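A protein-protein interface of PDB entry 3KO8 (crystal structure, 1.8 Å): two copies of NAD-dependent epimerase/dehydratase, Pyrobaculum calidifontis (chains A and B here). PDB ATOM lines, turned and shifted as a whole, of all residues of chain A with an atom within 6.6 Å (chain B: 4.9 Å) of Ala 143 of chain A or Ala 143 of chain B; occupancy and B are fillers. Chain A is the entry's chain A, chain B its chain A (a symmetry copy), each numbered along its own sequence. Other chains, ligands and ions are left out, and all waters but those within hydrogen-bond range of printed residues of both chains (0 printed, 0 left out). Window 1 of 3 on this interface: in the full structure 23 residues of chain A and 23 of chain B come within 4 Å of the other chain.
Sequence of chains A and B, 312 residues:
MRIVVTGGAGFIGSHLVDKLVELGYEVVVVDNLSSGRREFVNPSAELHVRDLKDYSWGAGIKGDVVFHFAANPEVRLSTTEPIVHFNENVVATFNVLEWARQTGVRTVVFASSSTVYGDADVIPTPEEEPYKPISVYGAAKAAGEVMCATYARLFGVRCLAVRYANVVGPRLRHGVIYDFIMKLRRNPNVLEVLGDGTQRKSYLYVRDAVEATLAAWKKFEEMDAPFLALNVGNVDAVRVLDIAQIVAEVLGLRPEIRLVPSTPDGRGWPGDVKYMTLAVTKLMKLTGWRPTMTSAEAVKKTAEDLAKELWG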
ATOM      1  N   VAL A  90      -5.590  25.603  12.196  1.00  0.00           N
ATOM      2  CA  VAL A  90      -6.313  25.237  10.989  1.00  0.00           C
ATOM      3  C   VAL A  90      -5.458  25.140   9.731  1.00  0.00           C
ATOM      4  O   VAL A  90      -5.529  24.126   9.022  1.00  0.00           O
ATOM      5  CB  VAL A  90      -7.484  26.224  10.708  1.00  0.00           C
ATOM      6  CG1 VAL A  90      -8.354  25.644   9.581  1.00  0.00           C
ATOM      7  CG2 VAL A  90      -8.348  26.396  11.955  1.00  0.00           C
ATOM      8  N   THR A  93      -2.880  22.270  10.131  1.00  0.00           N
ATOM      9  CA  THR A  93      -3.505  20.956  10.043  1.00  0.00           C
ATOM     10  C   THR A  93      -3.911  20.617   8.627  1.00  0.00           C
ATOM     11  O   THR A  93      -3.739  19.472   8.177  1.00  0.00           O
ATOM     12  CB  THR A  93      -4.723  20.883  10.982  1.00  0.00           C
ATOM     13  OG1 THR A  93      -4.250  21.004  12.335  1.00  0.00           O
ATOM     14  CG2 THR A  93      -5.447  19.517  10.823  1.00  0.00           C
ATOM     15  N   LEU A  97      -2.664  17.491   6.360  1.00  0.00           N
ATOM     16  CA  LEU A  97      -3.536  16.542   5.650  1.00  0.00           C
ATOM     17  C   LEU A  97      -3.208  16.450   4.144  1.00  0.00           C
ATOM     18  O   LEU A  97      -3.247  15.355   3.549  1.00  0.00           O
ATOM     19  CB  LEU A  97      -5.022  16.937   5.858  1.00  0.00           C
ATOM     20  CG  LEU A  97      -5.521  16.820   7.306  1.00  0.00           C
ATOM     21  CD1 LEU A  97      -6.923  17.491   7.455  1.00  0.00           C
ATOM     22  CD2 LEU A  97      -5.617  15.332   7.689  1.00  0.00           C
ATOM     23  N   PHE A 110      -4.397  12.741  15.330  1.00  0.00           N
ATOM     24  CA  PHE A 110      -4.467  14.202  15.581  1.00  0.00           C
ATOM     25  C   PHE A 110      -4.671  14.541  17.040  1.00  0.00           C
ATOM     26  O   PHE A 110      -5.585  14.018  17.672  1.00  0.00           O
ATOM     27  CB  PHE A 110      -5.638  14.764  14.741  1.00  0.00           C
ATOM     28  CG  PHE A 110      -5.920  16.260  14.955  1.00  0.00           C
ATOM     29  CD1 PHE A 110      -4.916  17.197  14.753  1.00  0.00           C
ATOM     30  CD2 PHE A 110      -7.204  16.701  15.281  1.00  0.00           C
ATOM     31  CE1 PHE A 110      -5.179  18.575  14.868  1.00  0.00           C
ATOM     32  CE2 PHE A 110      -7.495  18.054  15.394  1.00  0.00           C
ATOM     33  CZ  PHE A 110      -6.466  19.001  15.186  1.00  0.00           C
ATOM     34  N   VAL A 116     -12.873  21.618  22.224  1.00  0.00           N
ATOM     35  CA  VAL A 116     -13.831  21.564  21.129  1.00  0.00           C
ATOM     36  C   VAL A 116     -15.255  21.518  21.692  1.00  0.00           C
ATOM     37  O   VAL A 116     -16.205  21.869  20.989  1.00  0.00           O
ATOM     38  CB  VAL A 116     -13.616  20.335  20.192  1.00  0.00           C
ATOM     39  CG1 VAL A 116     -12.193  20.356  19.637  1.00  0.00           C
ATOM     40  CG2 VAL A 116     -13.914  19.008  20.927  1.00  0.00           C
ATOM     41  N   TYR A 131     -19.768  20.098  19.030  1.00  0.00           N
ATOM     42  CA  TYR A 131     -18.727  21.128  19.060  1.00  0.00           C
ATOM     43  C   TYR A 131     -19.411  22.429  19.475  1.00  0.00           C
ATOM     44  O   TYR A 131     -20.342  22.883  18.791  1.00  0.00           O
ATOM     45  CB  TYR A 131     -18.158  21.384  17.672  1.00  0.00           C
ATOM     46  CG  TYR A 131     -17.431  20.235  17.034  1.00  0.00           C
ATOM     47  CD1 TYR A 131     -16.411  19.560  17.722  1.00  0.00           C
ATOM     48  CD2 TYR A 131     -17.700  19.869  15.718  1.00  0.00           C
ATOM     49  CE1 TYR A 131     -15.688  18.566  17.113  1.00  0.00           C
ATOM     50  CE2 TYR A 131     -16.972  18.863  15.094  1.00  0.00           C
ATOM     51  CZ  TYR A 131     -15.964  18.214  15.802  1.00  0.00           C
ATOM     52  OH  TYR A 131     -15.225  17.205  15.200  1.00  0.00           O
ATOM     53  N   GLY A 138     -10.267  26.587  20.303  1.00  0.00           N
ATOM     54  CA  GLY A 138     -11.226  25.488  20.317  1.00  0.00           C
ATOM     55  C   GLY A 138     -11.899  25.313  18.974  1.00  0.00           C
ATOM     56  O   GLY A 138     -12.111  24.186  18.503  1.00  0.00           O
ATOM     57  N   ALA A 139     -12.260  26.427  18.342  1.00  0.00           N
ATOM     58  CA  ALA A 139     -12.889  26.363  17.030  1.00  0.00           C
ATOM     59  C   ALA A 139     -11.892  25.809  16.013  1.00  0.00           C
ATOM     60  O   ALA A 139     -12.263  25.037  15.093  1.00  0.00           O
ATOM     61  CB  ALA A 139     -13.331  27.768  16.584  1.00  0.00           C
ATOM     62  N   ALA A 140     -10.637  26.190  16.177  1.00  0.00           N
ATOM     63  CA  ALA A 140      -9.603  25.751  15.246  1.00  0.00           C
ATOM     64  C   ALA A 140      -9.401  24.235  15.380  1.00  0.00           C
ATOM     65  O   ALA A 140      -9.251  23.552  14.366  1.00  0.00           O
ATOM     66  CB  ALA A 140      -8.278  26.498  15.497  1.00  0.00           C
ATOM     67  N   LYS A 141      -9.382  23.717  16.606  1.00  0.00           N
ATOM     68  CA  LYS A 141      -9.232  22.260  16.786  1.00  0.00           C
ATOM     69  C   LYS A 141     -10.462  21.542  16.235  1.00  0.00           C
ATOM     70  O   LYS A 141     -10.356  20.482  15.612  1.00  0.00           O
ATOM     71  CB  LYS A 141      -9.037  21.906  18.266  1.00  0.00           C
ATOM     72  CG  LYS A 141      -7.684  22.314  18.816  1.00  0.00           C
ATOM     73  CD  LYS A 141      -6.590  21.520  18.107  1.00  0.00           C
ATOM     74  CE  LYS A 141      -5.244  21.656  18.865  1.00  0.00           C
ATOM     75  NZ  LYS A 141      -4.227  20.766  18.200  1.00  0.00           N
ATOM     76  N   ALA A 142     -11.645  22.104  16.439  1.00  0.00           N
ATOM     77  CA  ALA A 142     -12.829  21.442  15.893  1.00  0.00           C
ATOM     78  C   ALA A 142     -12.788  21.446  14.371  1.00  0.00           C
ATOM     79  O   ALA A 142     -13.109  20.444  13.733  1.00  0.00           O
ATOM     80  CB  ALA A 142     -14.134  22.121  16.405  1.00  0.00           C
ATOM     81  N   ALA A 143     -12.406  22.568  13.774  1.00  0.00           N
ATOM     82  CA  ALA A 143     -12.293  22.615  12.312  1.00  0.00           C
ATOM     83  C   ALA A 143     -11.228  21.600  11.853  1.00  0.00           C
ATOM     84  O   ALA A 143     -11.380  20.937  10.811  1.00  0.00           O
ATOM     85  CB  ALA A 143     -11.917  24.030  11.862  1.00  0.00           C
ATOM     86  N   GLY A 144     -10.145  21.487  12.614  1.00  0.00           N
ATOM     87  CA  GLY A 144      -9.133  20.510  12.249  1.00  0.00           C
ATOM     88  C   GLY A 144      -9.746  19.100  12.254  1.00  0.00           C
ATOM     89  O   GLY A 144      -9.499  18.294  11.342  1.00  0.00           O
ATOM     90  N   GLU A 145     -10.539  18.774  13.267  1.00  0.00           N
ATOM     91  CA  GLU A 145     -11.167  17.439  13.312  1.00  0.00           C
ATOM     92  C   GLU A 145     -12.077  17.224  12.098  1.00  0.00           C
ATOM     93  O   GLU A 145     -12.117  16.148  11.504  1.00  0.00           O
ATOM     94  CB  GLU A 145     -12.036  17.254  14.561  1.00  0.00           C
ATOM     95  CG  GLU A 145     -11.275  17.098  15.897  1.00  0.00           C
ATOM     96  CD  GLU A 145     -12.196  16.594  16.983  1.00  0.00           C
ATOM     97  OE1 GLU A 145     -13.338  16.207  16.649  1.00  0.00           O
ATOM     98  OE2 GLU A 145     -11.812  16.584  18.162  1.00  0.00           O
ATOM     99  N   VAL A 146     -12.860  18.239  11.751  1.00  0.00           N
ATOM    100  CA  VAL A 146     -13.785  18.102  10.622  1.00  0.00           C
ATOM    101  C   VAL A 146     -12.996  17.816   9.335  1.00  0.00           C
ATOM    102  O   VAL A 146     -13.354  16.943   8.525  1.00  0.00           O
ATOM    103  CB  VAL A 146     -14.605  19.392  10.482  1.00  0.00           C
ATOM    104  CG1 VAL A 146     -15.417  19.369   9.142  1.00  0.00           C
ATOM    105  CG2 VAL A 146     -15.558  19.481  11.683  1.00  0.00           C
ATOM    106  N   MET A 147     -11.904  18.536   9.141  1.00  0.00           N
ATOM    107  CA  MET A 147     -11.084  18.321   7.959  1.00  0.00           C
ATOM    108  C   MET A 147     -10.453  16.919   7.986  1.00  0.00           C
ATOM    109  O   MET A 147     -10.406  16.245   6.943  1.00  0.00           O
ATOM    110  CB  MET A 147      -9.976  19.392   7.840  1.00  0.00           C
ATOM    111  CG  MET A 147     -10.542  20.825   7.551  1.00  0.00           C
ATOM    112  SD  MET A 147      -9.182  21.973   7.135  1.00  0.00           S
ATOM    113  CE  MET A 147      -8.294  22.013   8.737  1.00  0.00           C
ATOM    114  N   CYS A 148      -9.956  16.500   9.155  1.00  0.00           N
ATOM    115  CA  CYS A 148      -9.345  15.159   9.273  1.00  0.00           C
ATOM    116  C   CYS A 148     -10.355  14.054   8.950  1.00  0.00           C
ATOM    117  O   CYS A 148     -10.034  13.095   8.223  1.00  0.00           O
ATOM    118  CB  CYS A 148      -8.824  14.902  10.687  1.00  0.00           C
ATOM    119  SG  CYS A 148      -7.288  15.804  11.111  1.00  0.00           S
ATOM    120  N   VAL B  90     -12.426  28.438   3.910  1.00  0.00           N
ATOM    121  CA  VAL B  90     -12.004  28.592   5.293  1.00  0.00           C
ATOM    122  C   VAL B  90     -11.205  29.856   5.586  1.00  0.00           C
ATOM    123  O   VAL B  90     -11.540  30.583   6.531  1.00  0.00           O
ATOM    124  CB  VAL B  90     -11.171  27.365   5.771  1.00  0.00           C
ATOM    125  CG1 VAL B  90     -10.978  27.469   7.292  1.00  0.00           C
ATOM    126  CG2 VAL B  90     -11.906  26.065   5.456  1.00  0.00           C
ATOM    127  N   ALA B 139     -16.279  20.186   3.904  1.00  0.00           N
ATOM    128  CA  ALA B 139     -15.551  20.320   5.158  1.00  0.00           C
ATOM    129  C   ALA B 139     -15.243  21.795   5.414  1.00  0.00           C
ATOM    130  O   ALA B 139     -15.285  22.276   6.574  1.00  0.00           O
ATOM    131  CB  ALA B 139     -14.228  19.537   5.090  1.00  0.00           C
ATOM    132  N   ALA B 140     -14.945  22.510   4.343  1.00  0.00           N
ATOM    133  CA  ALA B 140     -14.600  23.922   4.470  1.00  0.00           C
ATOM    134  C   ALA B 140     -15.831  24.712   4.936  1.00  0.00           C
ATOM    135  O   ALA B 140     -15.699  25.594   5.786  1.00  0.00           O
ATOM    136  CB  ALA B 140     -14.070  24.486   3.136  1.00  0.00           C
ATOM    137  N   LYS B 141     -17.006  24.414   4.384  1.00  0.00           N
ATOM    138  CA  LYS B 141     -18.225  25.117   4.828  1.00  0.00           C
ATOM    139  C   LYS B 141     -18.535  24.749   6.277  1.00  0.00           C
ATOM    140  O   LYS B 141     -18.944  25.594   7.077  1.00  0.00           O
ATOM    141  CB  LYS B 141     -19.419  24.766   3.931  1.00  0.00           C
ATOM    142  CG  LYS B 141     -19.336  25.372   2.543  1.00  0.00           C
ATOM    143  CD  LYS B 141     -19.400  26.893   2.651  1.00  0.00           C
ATOM    144  CE  LYS B 141     -19.658  27.523   1.259  1.00  0.00           C
ATOM    145  NZ  LYS B 141     -19.830  29.010   1.431  1.00  0.00           N
ATOM    146  N   ALA B 142     -18.336  23.492   6.648  1.00  0.00           N
ATOM    147  CA  ALA B 142     -18.602  23.130   8.040  1.00  0.00           C
ATOM    148  C   ALA B 142     -17.629  23.842   8.970  1.00  0.00           C
ATOM    149  O   ALA B 142     -18.022  24.340  10.026  1.00  0.00           O
ATOM    150  CB  ALA B 142     -18.520  21.587   8.242  1.00  0.00           C
ATOM    151  N   ALA B 143     -16.356  23.888   8.601  1.00  0.00           N
ATOM    152  CA  ALA B 143     -15.382  24.608   9.429  1.00  0.00           C
ATOM    153  C   ALA B 143     -15.776  26.097   9.497  1.00  0.00           C
ATOM    154  O   ALA B 143     -15.638  26.750  10.547  1.00  0.00           O
ATOM    155  CB  ALA B 143     -13.977  24.451   8.840  1.00  0.00           C
ATOM    156  N   GLY B 144     -16.251  26.639   8.381  1.00  0.00           N
ATOM    157  CA  GLY B 144     -16.681  28.027   8.407  1.00  0.00           C
ATOM    158  C   GLY B 144     -17.820  28.200   9.424  1.00  0.00           C
ATOM    159  O   GLY B 144     -17.838  29.167  10.202  1.00  0.00           O
ATOM    160  N   GLU B 145     -18.783  27.286   9.435  1.00  0.00           N
ATOM    161  CA  GLU B 145     -19.891  27.396  10.404  1.00  0.00           C
ATOM    162  C   GLU B 145     -19.366  27.340  11.842  1.00  0.00           C
ATOM    163  O   GLU B 145     -19.819  28.068  12.724  1.00  0.00           O
ATOM    164  CB  GLU B 145     -20.903  26.254  10.252  1.00  0.00           C
ATOM    165  CG  GLU B 145     -21.804  26.311   8.998  1.00  0.00           C
ATOM    166  CD  GLU B 145     -22.961  25.348   9.124  1.00  0.00           C
ATOM    167  OE1 GLU B 145     -23.146  24.798  10.232  1.00  0.00           O
ATOM    168  OE2 GLU B 145     -23.684  25.120   8.142  1.00  0.00           O
ATOM    169  N   VAL B 146     -18.436  26.428  12.103  1.00  0.00           N
ATOM    170  CA  VAL B 146     -17.906  26.287  13.462  1.00  0.00           C
ATOM    171  C   VAL B 146     -17.239  27.601  13.900  1.00  0.00           C
ATOM    172  O   VAL B 146     -17.426  28.088  15.028  1.00  0.00           O
ATOM    173  CB  VAL B 146     -16.898  25.129  13.493  1.00  0.00           C
ATOM    174  CG1 VAL B 146     -16.136  25.117  14.863  1.00  0.00           C
ATOM    175  CG2 VAL B 146     -17.675  23.819  13.302  1.00  0.00           C
ATOM    176  N   MET B 147     -16.468  28.196  13.007  1.00  0.00           N
ATOM    177  CA  MET B 147     -15.809  29.453  13.327  1.00  0.00           C
ATOM    178  C   MET B 147     -16.848  30.568  13.538  1.00  0.00           C
ATOM    179  O   MET B 147     -16.699  31.380  14.467  1.00  0.00           O
ATOM    180  CB  MET B 147     -14.815  29.866  12.219  1.00  0.00           C
ATOM    181  CG  MET B 147     -13.581  28.905  12.118  1.00  0.00           C
ATOM    182  SD  MET B 147     -12.316  29.610  11.003  1.00  0.00           S
ATOM    183  CE  MET B 147     -13.224  29.556   9.412  1.00  0.00           C
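Val 90 of chain A touches its own counterpart, Val 90 of chain B. Ala 139 of chain A touches Val 146 of chain B, and with the chains exchanged Val 146 of chain A touches Ala 139 of chain B. Ala 142 of chain A touches Val 146 of chain B, and with the chains exchanged Val 146 of chain A touches Ala 142 of chain B. Ala 143 of chain A touches its own counterpart, Ala 143 of chain B. Positions printed for both chains: 90, 139, 140, 141, 142, 143, 144, 145, 146 and 147. Of the 6 pairs that touch across the chains among the printed residues, 6 have their exchanged pair printed and touching as well.
Among the printed residues, pairs that only touch across the chains: Ala 143 of chain A with Ala 143 of chain B (3.7 Å), Ala 139 of chain A with Val 146 of chain B (3.9 Å), Val 146 of chain A with Ala 139 of chain B (3.9 Å), Val 146 of chain A with Ala 142 of chain B (3.9 Å), Ala 142 of chain A with Val 146 of chain B (3.9 Å) and Val 90 of chain A with Val 90 of chain B (3.9 Å).
Of the 10 printed residues of chain B, 5 touch a printed residue of chain A. Hydrophobic or aromatic side chains of chain B that line the printed part of chain A: Val 90, Ala 142, Ala 143 and Val 146.
Of the printed residues of chain B, Val 90 of chain A touches Val 90. Thr 93 of chain A touches none of the printed residues of chain B. Ala 143 of chain A touches just one residue of chain B: Ala 143. Of the printed residues of chain A, Ala 139 of chain B touches Val 146. Of chain A, only Ala 143 (3.7 Å) comes within 4 Å of Ala 143 of chain B. The nearest residue of chain B that does not touch Ala 143 of chain A is Val 146 of chain B (4.6 Å). The nearest residue of chain A that does not touch Ala 143 of chain B is Val 146 of chain A (4.6 Å). The nearest printed residue of chain B that does not touch Val 146 of chain A is Ala 143 of chain B (4.6 Å).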
